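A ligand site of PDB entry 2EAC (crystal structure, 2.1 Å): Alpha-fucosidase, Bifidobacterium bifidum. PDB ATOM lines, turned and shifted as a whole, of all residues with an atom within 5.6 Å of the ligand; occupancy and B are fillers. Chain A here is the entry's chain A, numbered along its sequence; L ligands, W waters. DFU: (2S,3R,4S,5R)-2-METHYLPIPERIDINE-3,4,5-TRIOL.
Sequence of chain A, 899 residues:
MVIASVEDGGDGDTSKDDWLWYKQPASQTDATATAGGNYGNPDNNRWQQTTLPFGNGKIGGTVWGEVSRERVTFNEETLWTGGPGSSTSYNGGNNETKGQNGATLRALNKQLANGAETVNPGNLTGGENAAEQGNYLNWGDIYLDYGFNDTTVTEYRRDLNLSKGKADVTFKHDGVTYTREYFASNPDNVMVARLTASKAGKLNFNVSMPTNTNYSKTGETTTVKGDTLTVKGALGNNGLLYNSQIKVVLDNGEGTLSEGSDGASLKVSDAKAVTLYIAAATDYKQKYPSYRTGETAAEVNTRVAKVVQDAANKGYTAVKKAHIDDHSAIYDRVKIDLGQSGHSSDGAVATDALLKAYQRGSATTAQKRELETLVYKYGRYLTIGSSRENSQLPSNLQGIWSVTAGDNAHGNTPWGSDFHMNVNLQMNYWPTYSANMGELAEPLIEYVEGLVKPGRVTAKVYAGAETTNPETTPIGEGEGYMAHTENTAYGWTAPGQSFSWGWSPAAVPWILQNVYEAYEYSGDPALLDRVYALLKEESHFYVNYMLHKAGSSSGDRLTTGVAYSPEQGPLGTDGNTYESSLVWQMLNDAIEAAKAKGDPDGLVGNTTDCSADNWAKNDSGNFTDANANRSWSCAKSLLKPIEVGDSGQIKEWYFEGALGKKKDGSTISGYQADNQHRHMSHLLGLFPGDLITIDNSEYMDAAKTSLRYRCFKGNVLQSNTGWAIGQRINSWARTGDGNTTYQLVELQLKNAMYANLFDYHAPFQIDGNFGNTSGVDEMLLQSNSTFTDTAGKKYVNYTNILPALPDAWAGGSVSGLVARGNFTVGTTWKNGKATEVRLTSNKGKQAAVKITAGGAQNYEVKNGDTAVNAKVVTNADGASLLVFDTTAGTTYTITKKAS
NH2 of Arg 678 is in salt-bridge range of OE2 of Glu 567 (3.2 Å).
The side-chain amide nitrogen (ND2) of Asn 424 sits at hydrogen-bond distance from the side-chain carboxylate (OD2) of Asp 767, at 2.7 Å.
The side-chain hydroxyl of Thr 721 lies within hydrogen-bond range of the indole nitrogen of Trp 723 (3.2 Å).
The side-chain carboxylate (OE1) of Glu 567 is in hydrogen-bond range of the side-chain amide nitrogen (ND2) of Asn 422, 2.9 Å away.
Water W1 lies within hydrogen-bond range of an oxygen (O4) of the ligand (2.6 Å), the side-chain amide nitrogen of Gln 765 (2.6 Å), the side-chain carboxylate of Asp 767 (2.6 Å) and the side-chain amide nitrogen of Asn 424 (3.0 Å).
An oxygen (O2) of the ligand lies within hydrogen-bond range of a ring nitrogen (NE2) of His 679 (2.7 Å).
NE2 of His 761 is in hydrogen-bond range of O3 of the ligand.
NH2 of Arg 678 lies within hydrogen-bond range of O2 of the ligand (2.8 Å).
The side-chain amide nitrogen (ND2) of Asn 424 is in hydrogen-bond range of an oxygen (O4) of the ligand, 2.9 Å away.
NE1 of Trp 723 is in hydrogen-bond range of O3 of the ligand, at 3.0 Å.
A nitrogen (N5) of the ligand lies within hydrogen-bond range of a ring nitrogen (ND1) of His 420 (3.2 Å).
OE2 of Glu 567 lies within hydrogen-bond range of O2 of the ligand (3.4 Å).
CD1 of Leu 397 touches C6 of the ligand, at 3.8 Å.
Trp 415 touches the ligand (CD2 to C6, 3.4 Å).
NE2 of Gln 765 touches C6 of the ligand, at 3.7 Å.
Hydrophobic or aromatic side chains that line the ligand: Leu 397, Trp 415, His 420, His 679, Trp 723 and His 761.
Ten residues have an atom within 4 Å of the ligand: Leu 397, Trp 415, His 420, Asn 424, Glu 567, Arg 678, His 679, Trp 723, His 761 and Gln 765.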
ATOM      1  N   LEU A 397      -6.913  20.507  23.393  1.00  0.00           N
ATOM      2  CA  LEU A 397      -6.982  20.163  21.942  1.00  0.00           C
ATOM      3  C   LEU A 397      -8.247  20.664  21.263  1.00  0.00           C
ATOM      4  O   LEU A 397      -8.287  20.768  20.014  1.00  0.00           O
ATOM      5  CB  LEU A 397      -6.912  18.654  21.721  1.00  0.00           C
ATOM      6  CG  LEU A 397      -5.553  17.979  21.865  1.00  0.00           C
ATOM      7  CD1 LEU A 397      -5.712  16.448  21.777  1.00  0.00           C
ATOM      8  CD2 LEU A 397      -4.550  18.477  20.765  1.00  0.00           C
ATOM      9  N   TRP A 415      -7.730  11.591  21.572  1.00  0.00           N
ATOM     10  CA  TRP A 415      -6.530  12.044  22.296  1.00  0.00           C
ATOM     11  C   TRP A 415      -6.865  12.753  23.626  1.00  0.00           C
ATOM     12  O   TRP A 415      -6.090  13.605  24.112  1.00  0.00           O
ATOM     13  CB  TRP A 415      -5.648  12.947  21.425  1.00  0.00           C
ATOM     14  CG  TRP A 415      -5.289  12.381  20.042  1.00  0.00           C
ATOM     15  CD1 TRP A 415      -4.345  11.422  19.761  1.00  0.00           C
ATOM     16  CD2 TRP A 415      -5.833  12.782  18.785  1.00  0.00           C
ATOM     17  NE1 TRP A 415      -4.291  11.207  18.397  1.00  0.00           N
ATOM     18  CE2 TRP A 415      -5.192  12.029  17.786  1.00  0.00           C
ATOM     19  CE3 TRP A 415      -6.807  13.722  18.404  1.00  0.00           C
ATOM     20  CZ2 TRP A 415      -5.517  12.163  16.426  1.00  0.00           C
ATOM     21  CZ3 TRP A 415      -7.121  13.853  17.072  1.00  0.00           C
ATOM     22  CH2 TRP A 415      -6.486  13.079  16.098  1.00  0.00           C
ATOM     23  N   HIS A 420      -1.396  18.638  24.505  1.00  0.00           N
ATOM     24  CA  HIS A 420      -0.548  17.813  23.692  1.00  0.00           C
ATOM     25  C   HIS A 420       0.647  18.671  23.250  1.00  0.00           C
ATOM     26  O   HIS A 420       0.486  19.609  22.458  1.00  0.00           O
ATOM     27  CB  HIS A 420      -1.350  17.338  22.479  1.00  0.00           C
ATOM     28  CG  HIS A 420      -1.373  15.852  22.313  1.00  0.00           C
ATOM     29  ND1 HIS A 420      -0.505  15.199  21.455  1.00  0.00           N
ATOM     30  CD2 HIS A 420      -2.151  14.904  22.877  1.00  0.00           C
ATOM     31  CE1 HIS A 420      -0.764  13.898  21.507  1.00  0.00           C
ATOM     32  NE2 HIS A 420      -1.749  13.698  22.358  1.00  0.00           N
ATOM     33  N   ASN A 422       3.671  18.139  21.760  1.00  0.00           N
ATOM     34  CA  ASN A 422       4.637  17.898  20.690  1.00  0.00           C
ATOM     35  C   ASN A 422       4.295  18.616  19.393  1.00  0.00           C
ATOM     36  O   ASN A 422       4.760  18.217  18.315  1.00  0.00           O
ATOM     37  CB  ASN A 422       4.965  16.400  20.451  1.00  0.00           C
ATOM     38  CG  ASN A 422       3.828  15.632  19.785  1.00  0.00           C
ATOM     39  OD1 ASN A 422       2.672  16.074  19.814  1.00  0.00           O
ATOM     40  ND2 ASN A 422       4.153  14.475  19.185  1.00  0.00           N
ATOM     41  N   VAL A 423       3.426  19.647  19.513  1.00  0.00           N
ATOM     42  CA  VAL A 423       3.110  20.667  18.471  1.00  0.00           C
ATOM     43  C   VAL A 423       1.772  21.365  18.784  1.00  0.00           C
ATOM     44  O   VAL A 423       1.606  22.534  18.465  1.00  0.00           O
ATOM     45  CB  VAL A 423       3.061  20.146  16.989  1.00  0.00           C
ATOM     46  CG1 VAL A 423       1.972  19.070  16.768  1.00  0.00           C
ATOM     47  CG2 VAL A 423       2.876  21.339  15.959  1.00  0.00           C
ATOM     48  N   ASN A 424       0.812  20.637  19.371  1.00  0.00           N
ATOM     49  CA  ASN A 424      -0.538  21.145  19.348  1.00  0.00           C
ATOM     50  C   ASN A 424      -0.790  22.287  20.324  1.00  0.00           C
ATOM     51  O   ASN A 424      -1.437  23.295  19.946  1.00  0.00           O
ATOM     52  CB  ASN A 424      -1.585  20.033  19.537  1.00  0.00           C
ATOM     53  CG  ASN A 424      -1.283  18.823  18.693  1.00  0.00           C
ATOM     54  OD1 ASN A 424      -0.458  17.999  19.064  1.00  0.00           O
ATOM     55  ND2 ASN A 424      -1.908  18.737  17.535  1.00  0.00           N
ATOM     56  N   GLU A 567       6.426  12.477  14.133  1.00  0.00           N
ATOM     57  CA  GLU A 567       6.160  11.163  14.709  1.00  0.00           C
ATOM     58  C   GLU A 567       6.440  10.136  13.589  1.00  0.00           C
ATOM     59  O   GLU A 567       5.547   9.486  13.092  1.00  0.00           O
ATOM     60  CB  GLU A 567       4.730  11.045  15.243  1.00  0.00           C
ATOM     61  CG  GLU A 567       4.505  11.735  16.622  1.00  0.00           C
ATOM     62  CD  GLU A 567       3.135  11.475  17.253  1.00  0.00           C
ATOM     63  OE1 GLU A 567       2.846  12.074  18.342  1.00  0.00           O
ATOM     64  OE2 GLU A 567       2.325  10.690  16.656  1.00  0.00           O
ATOM     65  N   ARG A 678       3.048  14.506   8.396  1.00  0.00           N
ATOM     66  CA  ARG A 678       2.331  15.660   8.900  1.00  0.00           C
ATOM     67  C   ARG A 678       3.224  16.576   9.743  1.00  0.00           C
ATOM     68  O   ARG A 678       3.135  17.807   9.628  1.00  0.00           O
ATOM     69  CB  ARG A 678       1.073  15.221   9.665  1.00  0.00           C
ATOM     70  CG  ARG A 678       1.299  14.239  10.829  1.00  0.00           C
ATOM     71  CD  ARG A 678      -0.054  13.567  11.259  1.00  0.00           C
ATOM     72  NE  ARG A 678       0.171  12.837  12.502  1.00  0.00           N
ATOM     73  CZ  ARG A 678       0.852  11.690  12.586  1.00  0.00           C
ATOM     74  NH1 ARG A 678       1.303  11.091  11.486  1.00  0.00           N
ATOM     75  NH2 ARG A 678       1.050  11.129  13.783  1.00  0.00           N
ATOM     76  N   HIS A 679       4.051  15.987  10.603  1.00  0.00           N
ATOM     77  CA  HIS A 679       5.017  16.740  11.435  1.00  0.00           C
ATOM     78  C   HIS A 679       6.189  17.198  10.562  1.00  0.00           C
ATOM     79  O   HIS A 679       6.548  16.529   9.578  1.00  0.00           O
ATOM     80  CB  HIS A 679       5.553  15.849  12.579  1.00  0.00           C
ATOM     81  CG  HIS A 679       4.543  15.523  13.643  1.00  0.00           C
ATOM     82  ND1 HIS A 679       4.459  16.218  14.837  1.00  0.00           N
ATOM     83  CD2 HIS A 679       3.579  14.570  13.696  1.00  0.00           C
ATOM     84  CE1 HIS A 679       3.476  15.717  15.566  1.00  0.00           C
ATOM     85  NE2 HIS A 679       2.932  14.717  14.908  1.00  0.00           N
ATOM     86  N   THR A 721      -3.453  17.111   7.557  1.00  0.00           N
ATOM     87  CA  THR A 721      -4.332  17.460   8.699  1.00  0.00           C
ATOM     88  C   THR A 721      -4.369  18.993   8.829  1.00  0.00           C
ATOM     89  O   THR A 721      -3.412  19.675   8.471  1.00  0.00           O
ATOM     90  CB  THR A 721      -3.806  16.845  10.021  1.00  0.00           C
ATOM     91  OG1 THR A 721      -2.606  17.515  10.412  1.00  0.00           O
ATOM     92  CG2 THR A 721      -3.469  15.373   9.868  1.00  0.00           C
ATOM     93  N   TRP A 723      -3.848  20.977  11.326  1.00  0.00           N
ATOM     94  CA  TRP A 723      -2.708  21.526  12.055  1.00  0.00           C
ATOM     95  C   TRP A 723      -1.410  21.444  11.226  1.00  0.00           C
ATOM     96  O   TRP A 723      -0.549  22.336  11.322  1.00  0.00           O
ATOM     97  CB  TRP A 723      -2.515  20.861  13.436  1.00  0.00           C
ATOM     98  CG  TRP A 723      -1.988  19.440  13.446  1.00  0.00           C
ATOM     99  CD1 TRP A 723      -2.722  18.281  13.626  1.00  0.00           C
ATOM    100  CD2 TRP A 723      -0.638  19.018  13.253  1.00  0.00           C
ATOM    101  NE1 TRP A 723      -1.906  17.175  13.545  1.00  0.00           N
ATOM    102  CE2 TRP A 723      -0.622  17.594  13.331  1.00  0.00           C
ATOM    103  CE3 TRP A 723       0.570  19.700  13.001  1.00  0.00           C
ATOM    104  CZ2 TRP A 723       0.540  16.846  13.193  1.00  0.00           C
ATOM    105  CZ3 TRP A 723       1.731  18.942  12.859  1.00  0.00           C
ATOM    106  CH2 TRP A 723       1.701  17.539  12.956  1.00  0.00           C
ATOM    107  N   HIS A 761      -8.826  17.593  11.853  1.00  0.00           N
ATOM    108  CA  HIS A 761      -7.692  16.739  11.639  1.00  0.00           C
ATOM    109  C   HIS A 761      -7.920  15.674  10.516  1.00  0.00           C
ATOM    110  O   HIS A 761      -7.003  15.497   9.716  1.00  0.00           O
ATOM    111  CB  HIS A 761      -7.300  16.156  13.011  1.00  0.00           C
ATOM    112  CG  HIS A 761      -6.132  15.223  12.985  1.00  0.00           C
ATOM    113  ND1 HIS A 761      -6.218  13.957  12.453  1.00  0.00           N
ATOM    114  CD2 HIS A 761      -4.891  15.337  13.512  1.00  0.00           C
ATOM    115  CE1 HIS A 761      -5.059  13.342  12.611  1.00  0.00           C
ATOM    116  NE2 HIS A 761      -4.237  14.157  13.262  1.00  0.00           N
ATOM    117  N   GLN A 765     -10.136  19.604  15.690  1.00  0.00           N
ATOM    118  CA  GLN A 765      -8.981  19.908  16.515  1.00  0.00           C
ATOM    119  C   GLN A 765      -8.781  21.394  16.370  1.00  0.00           C
ATOM    120  O   GLN A 765      -8.684  21.892  15.254  1.00  0.00           O
ATOM    121  CB  GLN A 765      -7.739  19.178  15.987  1.00  0.00           C
ATOM    122  CG  GLN A 765      -7.770  17.650  16.238  1.00  0.00           C
ATOM    123  CD  GLN A 765      -7.621  17.328  17.711  1.00  0.00           C
ATOM    124  OE1 GLN A 765      -8.623  17.065  18.436  1.00  0.00           O
ATOM    125  NE2 GLN A 765      -6.391  17.389  18.189  1.00  0.00           N
ATOM    126  N   ASP A 767      -6.245  23.304  17.216  1.00  0.00           N
ATOM    127  CA  ASP A 767      -4.893  23.755  16.882  1.00  0.00           C
ATOM    128  C   ASP A 767      -4.856  24.526  15.552  1.00  0.00           C
ATOM    129  O   ASP A 767      -4.298  25.620  15.507  1.00  0.00           O
ATOM    130  CB  ASP A 767      -3.873  22.589  16.861  1.00  0.00           C
ATOM    131  CG  ASP A 767      -4.437  21.293  16.226  1.00  0.00           C
ATOM    132  OD1 ASP A 767      -5.277  21.346  15.281  1.00  0.00           O
ATOM    133  OD2 ASP A 767      -3.985  20.217  16.702  1.00  0.00           O
HETATM  134  C1  DFU L   1      -0.138  13.794  17.674  1.00  0.00           C
HETATM  135  C2  DFU L   1      -0.253  14.137  16.191  1.00  0.00           C
HETATM  136  C3  DFU L   1      -1.697  13.937  15.706  1.00  0.00           C
HETATM  137  C4  DFU L   1      -2.674  14.765  16.536  1.00  0.00           C
HETATM  138  C5  DFU L   1      -2.536  14.409  18.038  1.00  0.00           C
HETATM  139  C6  DFU L   1      -3.462  15.267  18.906  1.00  0.00           C
HETATM  140  O4  DFU L   1      -2.381  16.176  16.377  1.00  0.00           O
HETATM  141  O3  DFU L   1      -1.782  14.319  14.324  1.00  0.00           O
HETATM  142  O2  DFU L   1       0.699  13.357  15.437  1.00  0.00           O
HETATM  143  N5  DFU L   1      -1.148  14.556  18.416  1.00  0.00           N
HETATM  144  O   HOH W   1      -4.509  17.639  16.410  1.00  0.00           O
